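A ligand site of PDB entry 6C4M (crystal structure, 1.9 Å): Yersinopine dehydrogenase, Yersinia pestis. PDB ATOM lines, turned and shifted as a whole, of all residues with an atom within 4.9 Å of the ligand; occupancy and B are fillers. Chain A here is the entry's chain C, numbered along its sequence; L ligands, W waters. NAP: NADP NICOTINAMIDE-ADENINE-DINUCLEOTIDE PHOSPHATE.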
ATOM      1  N   GLY A  29     -14.276 -26.764  18.357  1.00  0.00           N
ATOM      2  CA  GLY A  29     -14.213 -25.572  17.552  1.00  0.00           C
ATOM      3  C   GLY A  29     -12.891 -24.907  17.837  1.00  0.00           C
ATOM      4  O   GLY A  29     -12.519 -24.745  19.006  1.00  0.00           O
ATOM      5  N   ALA A  30     -12.152 -24.570  16.780  1.00  0.00           N
ATOM      6  CA  ALA A  30     -10.809 -24.027  16.889  1.00  0.00           C
ATOM      7  C   ALA A  30     -10.696 -22.690  16.173  1.00  0.00           C
ATOM      8  O   ALA A  30      -9.772 -22.478  15.374  1.00  0.00           O
ATOM      9  CB  ALA A  30      -9.796 -25.026  16.315  1.00  0.00           C
ATOM     10  N   GLY A  31     -11.641 -21.784  16.435  1.00  0.00           N
ATOM     11  CA  GLY A  31     -11.470 -20.387  16.110  1.00  0.00           C
ATOM     12  C   GLY A  31     -10.436 -19.739  17.019  1.00  0.00           C
ATOM     13  O   GLY A  31      -9.911 -20.360  17.958  1.00  0.00           O
ATOM     14  N   PRO A  32     -10.121 -18.469  16.775  1.00  0.00           N
ATOM     15  CA  PRO A  32      -9.061 -17.818  17.554  1.00  0.00           C
ATOM     16  C   PRO A  32      -9.352 -17.790  19.045  1.00  0.00           C
ATOM     17  O   PRO A  32      -8.415 -17.901  19.846  1.00  0.00           O
ATOM     18  CB  PRO A  32      -8.979 -16.396  16.951  1.00  0.00           C
ATOM     19  CG  PRO A  32     -10.215 -16.239  16.078  1.00  0.00           C
ATOM     20  CD  PRO A  32     -10.656 -17.592  15.701  1.00  0.00           C
ATOM     21  N   ALA A  33     -10.621 -17.673  19.444  1.00  0.00           N
ATOM     22  CA  ALA A  33     -10.951 -17.736  20.863  1.00  0.00           C
ATOM     23  C   ALA A  33     -10.462 -19.026  21.510  1.00  0.00           C
ATOM     24  O   ALA A  33     -10.062 -19.030  22.684  1.00  0.00           O
ATOM     25  CB  ALA A  33     -12.455 -17.579  21.048  1.00  0.00           C
ATOM     26  N   ALA A  34     -10.486 -20.141  20.776  1.00  0.00           N
ATOM     27  CA  ALA A  34     -10.065 -21.400  21.373  1.00  0.00           C
ATOM     28  C   ALA A  34      -8.600 -21.374  21.736  1.00  0.00           C
ATOM     29  O   ALA A  34      -8.181 -22.030  22.688  1.00  0.00           O
ATOM     30  CB  ALA A  34     -10.360 -22.572  20.430  1.00  0.00           C
ATOM     31  N   ASN A  53     -11.848 -29.352  15.126  1.00  0.00           N
ATOM     32  CA  ASN A  53     -12.276 -28.404  14.105  1.00  0.00           C
ATOM     33  C   ASN A  53     -12.751 -29.166  12.891  1.00  0.00           C
ATOM     34  O   ASN A  53     -12.128 -30.145  12.474  1.00  0.00           O
ATOM     35  CB  ASN A  53     -11.154 -27.439  13.697  1.00  0.00           C
ATOM     36  CG  ASN A  53     -11.683 -26.167  13.058  1.00  0.00           C
ATOM     37  OD1 ASN A  53     -11.738 -25.115  13.703  1.00  0.00           O
ATOM     38  ND2 ASN A  53     -12.081 -26.239  11.779  1.00  0.00           N
ATOM     39  N   ARG A  54     -13.853 -28.713  12.316  1.00  0.00           N
ATOM     40  CA  ARG A  54     -14.384 -29.321  11.109  1.00  0.00           C
ATOM     41  C   ARG A  54     -13.335 -29.278  10.008  1.00  0.00           C
ATOM     42  O   ARG A  54     -12.469 -28.383   9.996  1.00  0.00           O
ATOM     43  CB  ARG A  54     -15.640 -28.565  10.647  1.00  0.00           C
ATOM     44  CG  ARG A  54     -15.328 -27.140  10.267  1.00  0.00           C
ATOM     45  CD  ARG A  54     -16.532 -26.397   9.660  1.00  0.00           C
ATOM     46  NE  ARG A  54     -16.253 -24.963   9.533  1.00  0.00           N
ATOM     47  CZ  ARG A  54     -16.944 -24.134   8.740  1.00  0.00           C
ATOM     48  NH1 ARG A  54     -17.953 -24.596   8.025  1.00  0.00           N
ATOM     49  NH2 ARG A  54     -16.619 -22.846   8.675  1.00  0.00           N
ATOM     50  N   SER A  56     -12.791 -27.966   7.238  1.00  0.00           N
ATOM     51  CA  SER A  56     -12.656 -26.882   6.291  1.00  0.00           C
ATOM     52  C   SER A  56     -11.222 -26.825   5.780  1.00  0.00           C
ATOM     53  O   SER A  56     -10.360 -27.587   6.208  1.00  0.00           O
ATOM     54  CB  SER A  56     -13.036 -25.561   6.951  1.00  0.00           C
ATOM     55  OG  SER A  56     -12.212 -25.344   8.110  1.00  0.00           O
ATOM     56  N   LYS A  58      -9.220 -24.334   6.343  1.00  0.00           N
ATOM     57  CA  LYS A  58      -8.470 -23.886   7.535  1.00  0.00           C
ATOM     58  C   LYS A  58      -8.246 -25.027   8.517  1.00  0.00           C
ATOM     59  O   LYS A  58      -7.158 -25.186   9.082  1.00  0.00           O
ATOM     60  CB  LYS A  58      -9.213 -22.750   8.218  1.00  0.00           C
ATOM     61  CG  LYS A  58      -8.385 -22.020   9.292  1.00  0.00           C
ATOM     62  CD  LYS A  58      -9.181 -21.780  10.570  1.00  0.00           C
ATOM     63  CE  LYS A  58      -9.481 -23.076  11.332  1.00  0.00           C
ATOM     64  NZ  LYS A  58     -10.327 -22.824  12.526  1.00  0.00           N
ATOM     65  N   GLY A  59      -9.298 -25.821   8.780  1.00  0.00           N
ATOM     66  CA  GLY A  59      -9.150 -26.947   9.675  1.00  0.00           C
ATOM     67  C   GLY A  59      -8.114 -27.935   9.194  1.00  0.00           C
ATOM     68  O   GLY A  59      -7.273 -28.390   9.964  1.00  0.00           O
ATOM     69  N   ALA A 111     -16.953 -24.070  21.593  1.00  0.00           N
ATOM     70  CA  ALA A 111     -16.405 -22.844  21.051  1.00  0.00           C
ATOM     71  C   ALA A 111     -16.794 -22.617  19.602  1.00  0.00           C
ATOM     72  O   ALA A 111     -16.151 -21.814  18.927  1.00  0.00           O
ATOM     73  CB  ALA A 111     -14.876 -22.844  21.158  1.00  0.00           C
ATOM     74  N   VAL A 112     -17.824 -23.311  19.119  1.00  0.00           N
ATOM     75  CA  VAL A 112     -18.418 -23.014  17.815  1.00  0.00           C
ATOM     76  C   VAL A 112     -19.505 -21.966  18.069  1.00  0.00           C
ATOM     77  O   VAL A 112     -19.898 -21.780  19.242  1.00  0.00           O
ATOM     78  CB  VAL A 112     -19.016 -24.257  17.149  1.00  0.00           C
ATOM     79  CG1 VAL A 112     -17.944 -25.299  16.770  1.00  0.00           C
ATOM     80  CG2 VAL A 112     -20.122 -24.844  18.018  1.00  0.00           C
ATOM     81  N   PRO A 113     -20.051 -21.287  17.061  1.00  0.00           N
ATOM     82  CA  PRO A 113     -21.098 -20.301  17.334  1.00  0.00           C
ATOM     83  C   PRO A 113     -22.362 -20.985  17.839  1.00  0.00           C
ATOM     84  O   PRO A 113     -22.638 -22.150  17.510  1.00  0.00           O
ATOM     85  CB  PRO A 113     -21.338 -19.624  15.967  1.00  0.00           C
ATOM     86  CG  PRO A 113     -20.132 -19.956  15.159  1.00  0.00           C
ATOM     87  CD  PRO A 113     -19.676 -21.299  15.627  1.00  0.00           C
ATOM     88  N   ALA A 114     -23.144 -20.252  18.615  1.00  0.00           N
ATOM     89  CA  ALA A 114     -24.289 -20.867  19.269  1.00  0.00           C
ATOM     90  C   ALA A 114     -25.292 -21.461  18.281  1.00  0.00           C
ATOM     91  O   ALA A 114     -26.010 -22.399  18.627  1.00  0.00           O
ATOM     92  CB  ALA A 114     -25.020 -19.872  20.174  1.00  0.00           C
ATOM     93  N   HIS A 116     -24.806 -23.316  16.001  1.00  0.00           N
ATOM     94  CA  HIS A 116     -24.283 -24.615  15.590  1.00  0.00           C
ATOM     95  C   HIS A 116     -24.126 -25.574  16.762  1.00  0.00           C
ATOM     96  O   HIS A 116     -23.635 -26.697  16.571  1.00  0.00           O
ATOM     97  CB  HIS A 116     -22.928 -24.434  14.881  1.00  0.00           C
ATOM     98  CG  HIS A 116     -23.070 -23.878  13.499  1.00  0.00           C
ATOM     99  ND1 HIS A 116     -23.175 -24.681  12.387  1.00  0.00           N
ATOM    100  CD2 HIS A 116     -23.177 -22.595  13.047  1.00  0.00           C
ATOM    101  CE1 HIS A 116     -23.328 -23.931  11.312  1.00  0.00           C
ATOM    102  NE2 HIS A 116     -23.323 -22.661  11.689  1.00  0.00           N
ATOM    103  N   LEU A 138     -19.426 -21.469  25.423  1.00  0.00           N
ATOM    104  CA  LEU A 138     -18.457 -20.387  25.536  1.00  0.00           C
ATOM    105  C   LEU A 138     -19.089 -19.035  25.210  1.00  0.00           C
ATOM    106  O   LEU A 138     -18.757 -18.031  25.853  1.00  0.00           O
ATOM    107  CB  LEU A 138     -17.256 -20.668  24.643  1.00  0.00           C
ATOM    108  CG  LEU A 138     -16.104 -19.643  24.726  1.00  0.00           C
ATOM    109  CD1 LEU A 138     -15.430 -19.673  26.080  1.00  0.00           C
ATOM    110  CD2 LEU A 138     -15.057 -19.901  23.649  1.00  0.00           C
ATOM    111  N   SER A 139     -19.968 -18.976  24.209  1.00  0.00           N
ATOM    112  CA  SER A 139     -20.650 -17.736  23.836  1.00  0.00           C
ATOM    113  C   SER A 139     -22.098 -18.064  23.490  1.00  0.00           C
ATOM    114  O   SER A 139     -22.460 -18.227  22.316  1.00  0.00           O
ATOM    115  CB  SER A 139     -19.970 -17.009  22.692  1.00  0.00           C
ATOM    116  OG  SER A 139     -20.527 -15.702  22.569  1.00  0.00           O
ATOM    117  N   TYR A 168     -18.268 -14.648  24.761  1.00  0.00           N
ATOM    118  CA  TYR A 168     -16.836 -14.894  24.851  1.00  0.00           C
ATOM    119  C   TYR A 168     -16.202 -13.734  25.600  1.00  0.00           C
ATOM    120  O   TYR A 168     -16.682 -12.589  25.537  1.00  0.00           O
ATOM    121  CB  TYR A 168     -16.230 -15.064  23.451  1.00  0.00           C
ATOM    122  CG  TYR A 168     -14.735 -15.175  23.474  1.00  0.00           C
ATOM    123  CD1 TYR A 168     -14.098 -16.173  24.215  1.00  0.00           C
ATOM    124  CD2 TYR A 168     -13.929 -14.276  22.758  1.00  0.00           C
ATOM    125  CE1 TYR A 168     -12.722 -16.261  24.266  1.00  0.00           C
ATOM    126  CE2 TYR A 168     -12.550 -14.363  22.792  1.00  0.00           C
ATOM    127  CZ  TYR A 168     -11.950 -15.350  23.528  1.00  0.00           C
ATOM    128  OH  TYR A 168     -10.573 -15.430  23.556  1.00  0.00           O
ATOM    129  N   ALA A 170     -13.294 -12.152  25.565  1.00  0.00           N
ATOM    130  CA  ALA A 170     -12.206 -11.365  25.031  1.00  0.00           C
ATOM    131  C   ALA A 170     -12.484 -10.970  23.590  1.00  0.00           C
ATOM    132  O   ALA A 170     -13.541 -11.268  23.014  1.00  0.00           O
ATOM    133  CB  ALA A 170     -10.903 -12.133  25.106  1.00  0.00           C
ATOM    134  N   ASP A 171     -11.476 -10.341  22.995  1.00  0.00           N
ATOM    135  CA  ASP A 171     -11.409  -9.986  21.582  1.00  0.00           C
ATOM    136  C   ASP A 171     -10.128 -10.610  21.024  1.00  0.00           C
ATOM    137  O   ASP A 171      -9.026 -10.149  21.332  1.00  0.00           O
ATOM    138  CB  ASP A 171     -11.380  -8.465  21.435  1.00  0.00           C
ATOM    139  CG  ASP A 171     -11.428  -8.010  19.980  1.00  0.00           C
ATOM    140  OD1 ASP A 171     -11.009  -8.756  19.075  1.00  0.00           O
ATOM    141  OD2 ASP A 171     -11.912  -6.885  19.750  1.00  0.00           O
ATOM    142  N   THR A 172     -10.278 -11.667  20.231  1.00  0.00           N
ATOM    143  CA  THR A 172      -9.142 -12.482  19.804  1.00  0.00           C
ATOM    144  C   THR A 172      -9.246 -12.776  18.325  1.00  0.00           C
ATOM    145  O   THR A 172     -10.322 -13.123  17.830  1.00  0.00           O
ATOM    146  CB  THR A 172      -9.092 -13.825  20.583  1.00  0.00           C
ATOM    147  OG1 THR A 172      -9.143 -13.562  21.998  1.00  0.00           O
ATOM    148  CG2 THR A 172      -7.800 -14.591  20.245  1.00  0.00           C
ATOM    149  N   LYS A 173      -8.112 -12.691  17.629  1.00  0.00           N
ATOM    150  CA  LYS A 173      -8.069 -12.765  16.180  1.00  0.00           C
ATOM    151  C   LYS A 173      -6.804 -13.481  15.712  1.00  0.00           C
ATOM    152  O   LYS A 173      -5.805 -13.568  16.432  1.00  0.00           O
ATOM    153  CB  LYS A 173      -8.164 -11.361  15.557  1.00  0.00           C
ATOM    154  CG  LYS A 173      -9.574 -10.857  15.514  1.00  0.00           C
ATOM    155  CD  LYS A 173      -9.723  -9.459  16.115  1.00  0.00           C
ATOM    156  CE  LYS A 173     -11.196  -9.024  16.108  1.00  0.00           C
ATOM    157  NZ  LYS A 173     -12.100 -10.076  16.725  1.00  0.00           N
ATOM    158  N   TYR A 174      -6.863 -13.986  14.483  1.00  0.00           N
ATOM    159  CA  TYR A 174      -5.734 -14.680  13.894  1.00  0.00           C
ATOM    160  C   TYR A 174      -4.564 -13.742  13.585  1.00  0.00           C
ATOM    161  O   TYR A 174      -4.790 -12.627  13.129  1.00  0.00           O
ATOM    162  CB  TYR A 174      -6.188 -15.375  12.623  1.00  0.00           C
ATOM    163  CG  TYR A 174      -6.983 -16.627  12.886  1.00  0.00           C
ATOM    164  CD1 TYR A 174      -6.526 -17.580  13.782  1.00  0.00           C
ATOM    165  CD2 TYR A 174      -8.196 -16.862  12.234  1.00  0.00           C
ATOM    166  CE1 TYR A 174      -7.246 -18.735  14.005  1.00  0.00           C
ATOM    167  CE2 TYR A 174      -8.922 -18.010  12.469  1.00  0.00           C
ATOM    168  CZ  TYR A 174      -8.433 -18.944  13.361  1.00  0.00           C
ATOM    169  OH  TYR A 174      -9.128 -20.096  13.612  1.00  0.00           O
ATOM    170  N   ARG A 401     -20.908 -14.578   8.361  1.00  0.00           N
ATOM    171  CA  ARG A 401     -21.420 -14.985   9.664  1.00  0.00           C
ATOM    172  C   ARG A 401     -22.308 -13.906  10.259  1.00  0.00           C
ATOM    173  O   ARG A 401     -23.242 -14.200  11.021  1.00  0.00           O
ATOM    174  CB  ARG A 401     -20.280 -15.325  10.606  1.00  0.00           C
ATOM    175  CG  ARG A 401     -19.348 -14.156  10.891  1.00  0.00           C
ATOM    176  CD  ARG A 401     -18.760 -14.212  12.299  1.00  0.00           C
ATOM    177  NE  ARG A 401     -17.407 -14.742  12.295  1.00  0.00           N
ATOM    178  CZ  ARG A 401     -16.309 -13.997  12.224  1.00  0.00           C
ATOM    179  NH1 ARG A 401     -16.393 -12.671  12.137  1.00  0.00           N
ATOM    180  NH2 ARG A 401     -15.110 -14.594  12.229  1.00  0.00           N
ATOM    181  N   LEU A 404     -25.794 -14.300   9.125  1.00  0.00           N
ATOM    182  CA  LEU A 404     -26.272 -15.695   9.091  1.00  0.00           C
ATOM    183  C   LEU A 404     -26.512 -16.229  10.508  1.00  0.00           C
ATOM    184  O   LEU A 404     -27.565 -16.826  10.798  1.00  0.00           O
ATOM    185  CB  LEU A 404     -25.278 -16.578   8.352  1.00  0.00           C
ATOM    186  CG  LEU A 404     -25.657 -18.054   8.253  1.00  0.00           C
ATOM    187  CD1 LEU A 404     -26.941 -18.224   7.494  1.00  0.00           C
ATOM    188  CD2 LEU A 404     -24.547 -18.824   7.584  1.00  0.00           C
ATOM    189  N   GLU A 405     -25.535 -16.038  11.409  1.00  0.00           N
ATOM    190  CA  GLU A 405     -25.679 -16.505  12.788  1.00  0.00           C
ATOM    191  C   GLU A 405     -26.842 -15.789  13.491  1.00  0.00           C
ATOM    192  O   GLU A 405     -27.619 -16.428  14.220  1.00  0.00           O
ATOM    193  CB  GLU A 405     -24.368 -16.273  13.551  1.00  0.00           C
ATOM    194  CG  GLU A 405     -23.191 -17.209  13.151  1.00  0.00           C
ATOM    195  CD  GLU A 405     -21.854 -16.800  13.813  1.00  0.00           C
ATOM    196  OE1 GLU A 405     -21.884 -16.077  14.837  1.00  0.00           O
ATOM    197  OE2 GLU A 405     -20.786 -17.203  13.299  1.00  0.00           O
HETATM  198  PA  NAP L   1     -15.498 -18.618  14.901  1.00  0.00           P
HETATM  199  O1A NAP L   1     -16.721 -18.258  15.649  1.00  0.00           O
HETATM  200  O2A NAP L   1     -15.359 -17.794  13.594  1.00  0.00           O
HETATM  201  O5B NAP L   1     -15.585 -20.227  14.566  1.00  0.00           O
HETATM  202  C5B NAP L   1     -15.312 -21.092  15.695  1.00  0.00           C
HETATM  203  C4B NAP L   1     -15.372 -22.546  15.195  1.00  0.00           C
HETATM  204  O4B NAP L   1     -16.797 -22.747  14.609  1.00  0.00           O
HETATM  205  C3B NAP L   1     -14.541 -22.754  14.243  1.00  0.00           C
HETATM  206  O3B NAP L   1     -13.997 -24.112  14.319  1.00  0.00           O
HETATM  207  C2B NAP L   1     -15.417 -22.646  12.853  1.00  0.00           C
HETATM  208  O2B NAP L   1     -14.796 -23.454  11.796  1.00  0.00           O
HETATM  209  C1B NAP L   1     -16.577 -23.113  13.140  1.00  0.00           C
HETATM  210  N9A NAP L   1     -17.557 -22.308  12.418  1.00  0.00           N
HETATM  211  C8A NAP L   1     -17.766 -20.990  12.233  1.00  0.00           C
HETATM  212  N7A NAP L   1     -18.835 -20.905  11.436  1.00  0.00           N
HETATM  213  C5A NAP L   1     -19.259 -22.173  11.133  1.00  0.00           C
HETATM  214  C6A NAP L   1     -20.326 -22.553  10.361  1.00  0.00           C
HETATM  215  N6A NAP L   1     -21.343 -21.860   9.572  1.00  0.00           N
HETATM  216  N1A NAP L   1     -20.583 -23.870  10.201  1.00  0.00           N
HETATM  217  C2A NAP L   1     -19.786 -24.813  10.810  1.00  0.00           C
HETATM  218  N3A NAP L   1     -18.731 -24.425  11.581  1.00  0.00           N
HETATM  219  C4A NAP L   1     -18.471 -23.080  11.743  1.00  0.00           C
HETATM  220  O3  NAP L   1     -14.202 -18.312  15.877  1.00  0.00           O
HETATM  221  PN  NAP L   1     -14.108 -17.565  17.318  1.00  0.00           P
HETATM  222  O1N NAP L   1     -13.051 -18.276  18.031  1.00  0.00           O
HETATM  223  O2N NAP L   1     -13.758 -16.091  16.989  1.00  0.00           O
HETATM  224  O5D NAP L   1     -15.527 -17.528  18.196  1.00  0.00           O
HETATM  225  C5D NAP L   1     -15.792 -18.509  19.235  1.00  0.00           C
HETATM  226  C4D NAP L   1     -17.161 -18.145  19.841  1.00  0.00           C
HETATM  227  O4D NAP L   1     -17.085 -16.701  20.514  1.00  0.00           O
HETATM  228  C3D NAP L   1     -18.141 -18.059  18.954  1.00  0.00           C
HETATM  229  O3D NAP L   1     -19.399 -18.389  19.716  1.00  0.00           O
HETATM  230  C2D NAP L   1     -18.245 -16.583  18.558  1.00  0.00           C
HETATM  231  O2D NAP L   1     -19.541 -16.311  18.288  1.00  0.00           O
HETATM  232  C1D NAP L   1     -17.877 -15.878  19.879  1.00  0.00           C
HETATM  233  N1N NAP L   1     -17.168 -14.584  19.710  1.00  0.00           N
HETATM  234  C2N NAP L   1     -15.825 -14.505  19.585  1.00  0.00           C
HETATM  235  C3N NAP L   1     -15.221 -13.236  19.479  1.00  0.00           C
HETATM  236  C7N NAP L   1     -13.691 -13.099  19.320  1.00  0.00           C
HETATM  237  O7N NAP L   1     -13.128 -12.147  19.689  1.00  0.00           O
HETATM  238  N7N NAP L   1     -12.984 -14.197  18.721  1.00  0.00           N
HETATM  239  C4N NAP L   1     -15.980 -12.102  19.484  1.00  0.00           C
HETATM  240  C5N NAP L   1     -17.314 -12.182  19.605  1.00  0.00           C
HETATM  241  C6N NAP L   1     -17.920 -13.438  19.729  1.00  0.00           C
HETATM  242  P2B NAP L   1     -13.556 -22.793  10.850  1.00  0.00           P
HETATM  243  O1X NAP L   1     -14.214 -21.941   9.777  1.00  0.00           O
HETATM  244  O2X NAP L   1     -12.660 -21.934  11.687  1.00  0.00           O
HETATM  245  O3X NAP L   1     -12.806 -23.917  10.181  1.00  0.00           O
HETATM  246  O   HOH W   1     -22.337 -17.656  19.477  1.00  0.00           O
HETATM  247  O   HOH W   2     -22.264 -25.578   8.460  1.00  0.00           O
HETATM  248  O   HOH W   3     -15.318 -26.570  13.760  1.00  0.00           O
HETATM  249  O   HOH W   4     -13.341 -20.974  18.597  1.00  0.00           O
HETATM  250  O   HOH W   5     -18.817 -16.656  15.075  1.00  0.00           O
HETATM  251  O   HOH W   6     -17.998 -26.703  13.237  1.00  0.00           O
HETATM  252  O   HOH W   7     -19.746 -20.830  21.936  1.00  0.00           O
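The side-chain amino group (NZ) of Lys 58 lies within salt-bridge range of an oxygen (O2X) of the ligand (2.6 Å). An oxygen (O3B) of the ligand sits at hydrogen-bond distance from the side-chain amide oxygen of Asn 53 (2.5 Å). A ring nitrogen (NE2) of His 116 sits at hydrogen-bond distance from a nitrogen (N6A) of the ligand (3.0 Å). The backbone NH of Ala 30 is in hydrogen-bond range of an oxygen (O3B) of the ligand. The backbone carbonyl oxygen (O) of Thr 172 lies within hydrogen-bond range of a nitrogen (N7N) of the ligand (3.0 Å). O3D of the ligand sits at hydrogen-bond distance from O of Val 112 (3.5 Å). The side-chain hydroxyl (OG) of Ser 56 sits at hydrogen-bond distance from an oxygen (O3X) of the ligand. O2A of the ligand lies within salt-bridge range of NH2 of Arg 401, at 3.5 Å. The guanidinium group (NH2) of Arg 54 is in salt-bridge range of an oxygen (O1X) of the ligand, at 2.8 Å. N of Ala 33 lies within hydrogen-bond range of O1N of the ligand (2.9 Å). The backbone NH (N) of Thr 172 is in hydrogen-bond range of an oxygen (O7N) of the ligand (2.9 Å).
OD1 of Asp 171 lies within salt-bridge range of NZ of Lys 173 (2.9 Å). The side-chain amino group of Lys 58 lies within hydrogen-bond range of the backbone carbonyl oxygen of Ala 30, 2.9 Å away. The side-chain hydroxyl (OG) of Ser 139 lies within hydrogen-bond range of the backbone NH (N) of Tyr 168 (3.3 Å). The side-chain hydroxyl (OH) of Tyr 174 sits at hydrogen-bond distance from the backbone carbonyl oxygen (O) of Ala 30. NZ of Lys 58 lies within hydrogen-bond range of OH of Tyr 174, at 3.2 Å. OG1 of Thr 172 sits at hydrogen-bond distance from OH of Tyr 168 (2.8 Å). The side-chain amino group (NZ) of Lys 58 sits at hydrogen-bond distance from the side-chain amide oxygen (OD1) of Asn 53 (2.9 Å). The side-chain hydroxyl of Ser 56 lies within hydrogen-bond range of the backbone NH of Gly 59 (3.0 Å).
N of Pro 32 sits close to O1N of the ligand (3.2 Å). The backbone carbonyl oxygen (O) of Ala 170 lies close to an oxygen (O7N) of the ligand, 3.5 Å away. Gly 29 touches the ligand (CA to O3B, 3.6 Å). Gly 31 touches the ligand. O of Ala 111 touches C5D of the ligand, 3.3 Å away. Pro 113 touches the ligand. Ser 139 touches the ligand (CB to O3D, 3.3 Å). Tyr 168 touches the ligand (CB to O4D, 3.5 Å). Asp 171 touches the ligand (CA to O7N, 3.3 Å). NZ of Lys 173 touches O7N of the ligand (3.8 Å). Within 4 Å of the ligand: Gly 29, Ala 30, Gly 31, Pro 32, Ala 33, Asn 53, Arg 54, Ser 56, Lys 58, Ala 111, Val 112, Pro 113, His 116, Ser 139, Tyr 168, Ala 170, Asp 171, Thr 172, Lys 173 and Arg 401.
Water W5 bridges O1A of the ligand and OE2 of Glu 405. Water W4 lies within hydrogen-bond range of O1N of the ligand, N of Gly 31 and O of Ala 111. Water W3 lies within hydrogen-bond range of O3B of the ligand and N of Arg 54. Water W1 lies within hydrogen-bond range of N of Ala 114 (2.9 Å), O of Ser 139 (2.9 Å) and O3D of the ligand (3.0 Å). Water W7 lies within hydrogen-bond range of the backbone carbonyl oxygen of Val 112 (2.9 Å), the backbone NH of Ser 139 (2.9 Å) and an oxygen (O3D) of the ligand (3.3 Å).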
